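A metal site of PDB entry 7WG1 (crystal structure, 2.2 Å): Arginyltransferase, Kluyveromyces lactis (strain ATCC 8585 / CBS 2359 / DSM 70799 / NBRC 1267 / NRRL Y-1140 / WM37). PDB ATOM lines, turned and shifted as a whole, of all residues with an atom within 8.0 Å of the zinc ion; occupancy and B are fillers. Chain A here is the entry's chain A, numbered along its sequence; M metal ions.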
ATOM      1  N   ALA A  23      -9.286  24.721  29.472  1.00  0.00           N
ATOM      2  CA  ALA A  23      -8.567  24.992  28.225  1.00  0.00           C
ATOM      3  C   ALA A  23      -9.483  24.856  27.007  1.00  0.00           C
ATOM      4  O   ALA A  23      -9.339  25.587  26.007  1.00  0.00           O
ATOM      5  CB  ALA A  23      -7.367  24.053  28.112  1.00  0.00           C
ATOM      6  N   ASP A  24     -10.385  23.888  27.036  1.00  0.00           N
ATOM      7  CA  ASP A  24     -11.532  23.870  26.132  1.00  0.00           C
ATOM      8  C   ASP A  24     -12.573  24.783  26.761  1.00  0.00           C
ATOM      9  O   ASP A  24     -13.188  24.400  27.756  1.00  0.00           O
ATOM     10  CB  ASP A  24     -12.027  22.445  25.969  1.00  0.00           C
ATOM     11  CG  ASP A  24     -13.212  22.319  25.017  1.00  0.00           C
ATOM     12  OD1 ASP A  24     -13.678  23.349  24.466  1.00  0.00           O
ATOM     13  OD2 ASP A  24     -13.672  21.169  24.839  1.00  0.00           O
ATOM     14  N   LYS A  26     -10.642  28.025  26.472  1.00  0.00           N
ATOM     15  CA  LYS A  26      -9.887  29.263  26.718  1.00  0.00           C
ATOM     16  C   LYS A  26      -8.545  29.303  25.980  1.00  0.00           C
ATOM     17  O   LYS A  26      -8.097  30.392  25.590  1.00  0.00           O
ATOM     18  CB  LYS A  26      -9.665  29.456  28.217  1.00  0.00           C
ATOM     19  CG  LYS A  26      -9.129  30.846  28.628  1.00  0.00           C
ATOM     20  CD  LYS A  26      -8.686  30.838  30.117  1.00  0.00           C
ATOM     21  CE  LYS A  26      -8.299  32.234  30.661  1.00  0.00           C
ATOM     22  NZ  LYS A  26      -6.796  32.396  30.848  1.00  0.00           N
ATOM     23  N   CYS A  27      -7.872  28.158  25.824  1.00  0.00           N
ATOM     24  CA  CYS A  27      -6.585  28.144  25.112  1.00  0.00           C
ATOM     25  C   CYS A  27      -6.802  28.215  23.596  1.00  0.00           C
ATOM     26  O   CYS A  27      -7.404  27.312  23.006  1.00  0.00           O
ATOM     27  CB  CYS A  27      -5.774  26.884  25.441  1.00  0.00           C
ATOM     28  SG  CYS A  27      -4.106  26.919  24.724  1.00  0.00           S
ATOM     29  N   GLY A  28      -6.285  29.265  22.970  1.00  0.00           N
ATOM     30  CA  GLY A  28      -6.252  29.384  21.524  1.00  0.00           C
ATOM     31  C   GLY A  28      -5.147  28.632  20.812  1.00  0.00           C
ATOM     32  O   GLY A  28      -5.071  28.690  19.580  1.00  0.00           O
ATOM     33  N   TYR A  29      -4.272  27.926  21.525  1.00  0.00           N
ATOM     34  CA  TYR A  29      -3.234  27.142  20.864  1.00  0.00           C
ATOM     35  C   TYR A  29      -3.609  25.665  20.711  1.00  0.00           C
ATOM     36  O   TYR A  29      -3.276  25.048  19.689  1.00  0.00           O
ATOM     37  CB  TYR A  29      -1.929  27.252  21.639  1.00  0.00           C
ATOM     38  CG  TYR A  29      -1.522  28.676  21.989  1.00  0.00           C
ATOM     39  CD1 TYR A  29      -1.163  29.568  21.004  1.00  0.00           C
ATOM     40  CD2 TYR A  29      -1.470  29.094  23.316  1.00  0.00           C
ATOM     41  CE1 TYR A  29      -0.772  30.860  21.308  1.00  0.00           C
ATOM     42  CE2 TYR A  29      -1.083  30.393  23.632  1.00  0.00           C
ATOM     43  CZ  TYR A  29      -0.713  31.279  22.612  1.00  0.00           C
ATOM     44  OH  TYR A  29      -0.316  32.586  22.884  1.00  0.00           O
ATOM     45  N   CYS A  30      -4.299  25.089  21.698  1.00  0.00           N
ATOM     46  CA  CYS A  30      -4.698  23.687  21.662  1.00  0.00           C
ATOM     47  C   CYS A  30      -6.188  23.490  21.817  1.00  0.00           C
ATOM     48  O   CYS A  30      -6.651  22.366  21.715  1.00  0.00           O
ATOM     49  CB  CYS A  30      -3.995  22.914  22.796  1.00  0.00           C
ATOM     50  SG  CYS A  30      -4.781  23.185  24.458  1.00  0.00           S
ATOM     51  N   ASN A  31      -6.952  24.546  22.101  1.00  0.00           N
ATOM     52  CA  ASN A  31      -8.396  24.455  22.331  1.00  0.00           C
ATOM     53  C   ASN A  31      -8.766  23.345  23.306  1.00  0.00           C
ATOM     54  O   ASN A  31      -9.878  22.828  23.264  1.00  0.00           O
ATOM     55  CB  ASN A  31      -9.151  24.247  21.004  1.00  0.00           C
ATOM     56  CG  ASN A  31      -8.574  25.079  19.849  1.00  0.00           C
ATOM     57  OD1 ASN A  31      -7.977  24.532  18.914  1.00  0.00           O
ATOM     58  ND2 ASN A  31      -8.771  26.398  19.904  1.00  0.00           N
ATOM     59  N   GLY A  32      -7.848  22.982  24.217  1.00  0.00           N
ATOM     60  CA  GLY A  32      -8.080  21.912  25.171  1.00  0.00           C
ATOM     61  C   GLY A  32      -7.843  20.502  24.645  1.00  0.00           C
ATOM     62  O   GLY A  32      -8.016  19.534  25.396  1.00  0.00           O
ATOM     63  N   LYS A  33      -7.447  20.366  23.381  1.00  0.00           N
ATOM     64  CA  LYS A  33      -7.229  19.069  22.752  1.00  0.00           C
ATOM     65  C   LYS A  33      -5.742  18.738  22.849  1.00  0.00           C
ATOM     66  O   LYS A  33      -4.927  19.335  22.149  1.00  0.00           O
ATOM     67  CB  LYS A  33      -7.664  19.061  21.291  1.00  0.00           C
ATOM     68  CG  LYS A  33      -9.191  19.083  21.019  1.00  0.00           C
ATOM     69  CD  LYS A  33      -9.754  20.505  20.777  1.00  0.00           C
ATOM     70  CE  LYS A  33     -11.221  20.601  21.196  1.00  0.00           C
ATOM     71  NZ  LYS A  33     -11.808  21.989  21.160  1.00  0.00           N
ATOM     72  N   LYS A  34      -5.399  17.756  23.675  1.00  0.00           N
ATOM     73  CA  LYS A  34      -4.032  17.305  23.792  1.00  0.00           C
ATOM     74  C   LYS A  34      -3.951  15.794  23.626  1.00  0.00           C
ATOM     75  O   LYS A  34      -4.751  15.058  24.217  1.00  0.00           O
ATOM     76  CB  LYS A  34      -3.460  17.747  25.131  1.00  0.00           C
ATOM     77  CG  LYS A  34      -3.197  19.264  25.207  1.00  0.00           C
ATOM     78  CD  LYS A  34      -1.719  19.562  25.043  1.00  0.00           C
ATOM     79  CE  LYS A  34      -1.521  20.892  24.433  1.00  0.00           C
ATOM     80  NZ  LYS A  34      -0.257  20.924  23.688  1.00  0.00           N
ATOM     81  N   LEU A  58      -7.911  19.749  31.537  1.00  0.00           N
ATOM     82  CA  LEU A  58      -6.860  20.709  31.259  1.00  0.00           C
ATOM     83  C   LEU A  58      -7.337  22.134  31.506  1.00  0.00           C
ATOM     84  O   LEU A  58      -8.451  22.526  31.103  1.00  0.00           O
ATOM     85  CB  LEU A  58      -6.407  20.590  29.799  1.00  0.00           C
ATOM     86  CG  LEU A  58      -5.676  19.301  29.415  1.00  0.00           C
ATOM     87  CD1 LEU A  58      -5.334  19.292  27.913  1.00  0.00           C
ATOM     88  CD2 LEU A  58      -4.441  19.087  30.265  1.00  0.00           C
ATOM     89  N   GLN A  59      -6.497  22.901  32.168  1.00  0.00           N
ATOM     90  CA  GLN A  59      -6.743  24.300  32.465  1.00  0.00           C
ATOM     91  C   GLN A  59      -5.800  25.176  31.647  1.00  0.00           C
ATOM     92  O   GLN A  59      -4.665  24.796  31.339  1.00  0.00           O
ATOM     93  CB  GLN A  59      -6.559  24.580  33.972  1.00  0.00           C
ATOM     94  CG  GLN A  59      -7.559  23.860  34.902  1.00  0.00           C
ATOM     95  CD  GLN A  59      -9.025  24.239  34.633  1.00  0.00           C
ATOM     96  OE1 GLN A  59      -9.456  25.384  34.868  1.00  0.00           O
ATOM     97  NE2 GLN A  59      -9.787  23.281  34.133  1.00  0.00           N
ATOM     98  N   SER A  60      -6.306  26.338  31.244  1.00  0.00           N
ATOM     99  CA  SER A  60      -5.484  27.411  30.700  1.00  0.00           C
ATOM    100  C   SER A  60      -5.435  28.522  31.746  1.00  0.00           C
ATOM    101  O   SER A  60      -6.483  29.025  32.182  1.00  0.00           O
ATOM    102  CB  SER A  60      -6.048  27.933  29.379  1.00  0.00           C
ATOM    103  OG  SER A  60      -5.328  29.067  28.924  1.00  0.00           O
ATOM    104  N   SER A  61      -4.233  28.918  32.130  1.00  0.00           N
ATOM    105  CA  SER A  61      -4.023  29.728  33.315  1.00  0.00           C
ATOM    106  C   SER A  61      -3.012  30.819  33.027  1.00  0.00           C
ATOM    107  O   SER A  61      -1.914  30.520  32.546  1.00  0.00           O
ATOM    108  CB  SER A  61      -3.510  28.842  34.440  1.00  0.00           C
ATOM    109  OG  SER A  61      -2.782  27.787  33.862  1.00  0.00           O
ATOM    110  N   ASN A  98      -0.564  24.943  33.106  1.00  0.00           N
ATOM    111  CA  ASN A  98      -1.131  25.265  31.815  1.00  0.00           C
ATOM    112  C   ASN A  98      -1.198  24.050  30.915  1.00  0.00           C
ATOM    113  O   ASN A  98      -0.380  23.118  31.000  1.00  0.00           O
ATOM    114  CB  ASN A  98      -0.316  26.351  31.137  1.00  0.00           C
ATOM    115  CG  ASN A  98      -1.122  27.133  30.164  1.00  0.00           C
ATOM    116  OD1 ASN A  98      -2.169  27.668  30.506  1.00  0.00           O
ATOM    117  ND2 ASN A  98      -0.663  27.211  28.935  1.00  0.00           N
ATOM    118  N   CYS A  99      -2.207  24.064  30.021  1.00  0.00           N
ATOM    119  CA  CYS A  99      -2.333  23.006  29.025  1.00  0.00           C
ATOM    120  C   CYS A  99      -1.102  22.954  28.127  1.00  0.00           C
ATOM    121  O   CYS A  99      -0.530  21.904  27.916  1.00  0.00           O
ATOM    122  CB  CYS A  99      -3.570  23.227  28.187  1.00  0.00           C
ATOM    123  SG  CYS A  99      -3.726  24.947  27.696  1.00  0.00           S
ATOM    124  N   CYS A 100      -0.644  24.108  27.685  1.00  0.00           N
ATOM    125  CA  CYS A 100       0.501  24.241  26.786  1.00  0.00           C
ATOM    126  C   CYS A 100       1.697  24.836  27.522  1.00  0.00           C
ATOM    127  O   CYS A 100       1.535  25.716  28.379  1.00  0.00           O
ATOM    128  CB  CYS A 100       0.118  25.107  25.565  1.00  0.00           C
ATOM    129  SG  CYS A 100      -1.217  24.314  24.514  1.00  0.00           S
ATOM    130  N   ARG A 101       2.887  24.346  27.199  1.00  0.00           N
ATOM    131  CA  ARG A 101       4.134  24.822  27.816  1.00  0.00           C
ATOM    132  C   ARG A 101       4.675  25.937  26.933  1.00  0.00           C
ATOM    133  O   ARG A 101       5.170  25.689  25.809  1.00  0.00           O
ATOM    134  CB  ARG A 101       5.142  23.682  27.952  1.00  0.00           C
ATOM    135  CG  ARG A 101       6.087  23.767  29.157  1.00  0.00           C
ATOM    136  CD  ARG A 101       5.325  23.524  30.494  1.00  0.00           C
ATOM    137  NE  ARG A 101       4.575  22.273  30.383  1.00  0.00           N
ATOM    138  CZ  ARG A 101       3.280  22.101  30.581  1.00  0.00           C
ATOM    139  NH1 ARG A 101       2.525  23.047  31.097  1.00  0.00           N
ATOM    140  NH2 ARG A 101       2.736  20.936  30.239  1.00  0.00           N
ATOM    141  N   LEU A 102       4.567  27.176  27.407  1.00  0.00           N
ATOM    142  CA  LEU A 102       5.030  28.356  26.659  1.00  0.00           C
ATOM    143  C   LEU A 102       6.400  28.798  27.160  1.00  0.00           C
ATOM    144  O   LEU A 102       6.562  29.072  28.347  1.00  0.00           O
ATOM    145  CB  LEU A 102       4.042  29.503  26.833  1.00  0.00           C
ATOM    146  CG  LEU A 102       2.803  29.393  25.942  1.00  0.00           C
ATOM    147  CD1 LEU A 102       1.909  28.197  26.312  1.00  0.00           C
ATOM    148  CD2 LEU A 102       1.994  30.702  25.994  1.00  0.00           C
ATOM    149  N   ILE A 299       5.934  27.332  21.592  1.00  0.00           N
ATOM    150  CA  ILE A 299       5.265  26.124  22.036  1.00  0.00           C
ATOM    151  C   ILE A 299       5.679  25.016  21.082  1.00  0.00           C
ATOM    152  O   ILE A 299       5.321  25.048  19.894  1.00  0.00           O
ATOM    153  CB  ILE A 299       3.745  26.276  22.033  1.00  0.00           C
ATOM    154  CG1 ILE A 299       3.315  27.543  22.749  1.00  0.00           C
ATOM    155  CG2 ILE A 299       3.142  25.033  22.664  1.00  0.00           C
ATOM    156  CD1 ILE A 299       1.814  27.759  22.723  1.00  0.00           C
ATOM    157  N   ASP A 301       4.781  21.935  20.510  1.00  0.00           N
ATOM    158  CA  ASP A 301       3.779  21.116  19.844  1.00  0.00           C
ATOM    159  C   ASP A 301       2.659  21.897  19.141  1.00  0.00           C
ATOM    160  O   ASP A 301       1.695  21.279  18.687  1.00  0.00           O
ATOM    161  CB  ASP A 301       3.164  20.115  20.842  1.00  0.00           C
ATOM    162  CG  ASP A 301       2.356  20.770  21.979  1.00  0.00           C
ATOM    163  OD1 ASP A 301       1.917  21.938  21.849  1.00  0.00           O
ATOM    164  OD2 ASP A 301       2.136  20.051  22.993  1.00  0.00           O
ATOM    165  N   CYS A 302       2.766  23.235  19.004  1.00  0.00           N
ATOM    166  CA  CYS A 302       1.694  24.023  18.402  1.00  0.00           C
ATOM    167  C   CYS A 302       2.222  24.624  17.100  1.00  0.00           C
ATOM    168  O   CYS A 302       3.136  25.467  17.154  1.00  0.00           O
ATOM    169  CB  CYS A 302       1.210  25.130  19.347  1.00  0.00           C
ATOM    170  SG  CYS A 302       0.112  26.407  18.616  1.00  0.00           S
ATOM    171  N   ASN A 336       5.871  18.490  25.410  1.00  0.00           N
ATOM    172  CA  ASN A 336       5.131  19.517  26.158  1.00  0.00           C
ATOM    173  C   ASN A 336       5.631  19.542  27.609  1.00  0.00           C
ATOM    174  O   ASN A 336       4.901  19.966  28.505  1.00  0.00           O
ATOM    175  CB  ASN A 336       3.621  19.289  26.075  1.00  0.00           C
ATOM    176  CG  ASN A 336       2.788  20.577  26.334  1.00  0.00           C
ATOM    177  OD1 ASN A 336       3.109  21.666  25.826  1.00  0.00           O
ATOM    178  ND2 ASN A 336       1.696  20.439  27.100  1.00  0.00           N
HETATM  179 ZN    ZN M   1      -3.311  24.829  25.416  1.00  0.00          ZN
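The zinc ion is bound by SG of Cys 99 (2.3 Å), SG of Cys 100 (2.3 Å), SG of Cys 27 (2.3 Å) and SG of Cys 30 (2.4 Å).
The zinc ion has four donor atoms within binding distance.
The backbone NH (N) of Cys 99 sits at hydrogen-bond distance from the backbone carbonyl oxygen (O) of Gln 59, 2.9 Å away.
The backbone carbonyl oxygen (O) of Cys 99 is in hydrogen-bond range of the side-chain amide nitrogen (ND2) of Asn 336 (2.8 Å).
The side-chain amino group (NZ) of Lys 34 lies close to the side-chain sulfur (SG) of Cys 100.
The backbone carbonyl oxygen of Cys 100 is in hydrogen-bond range of the side-chain amide nitrogen of Asn 98.
The side-chain sulfur (SG) of Cys 27 sits close to the backbone NH (N) of Tyr 29 (3.4 Å).
SG of Cys 30 lies close to N of Gly 32 (3.1 Å).
Four residues have an atom within 4 Å of the zinc ion: Cys 27, Cys 30, Cys 99 and Cys 100.
The nearest printed residue that does not touch the zinc ion is Lys 34 (4.4 Å).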
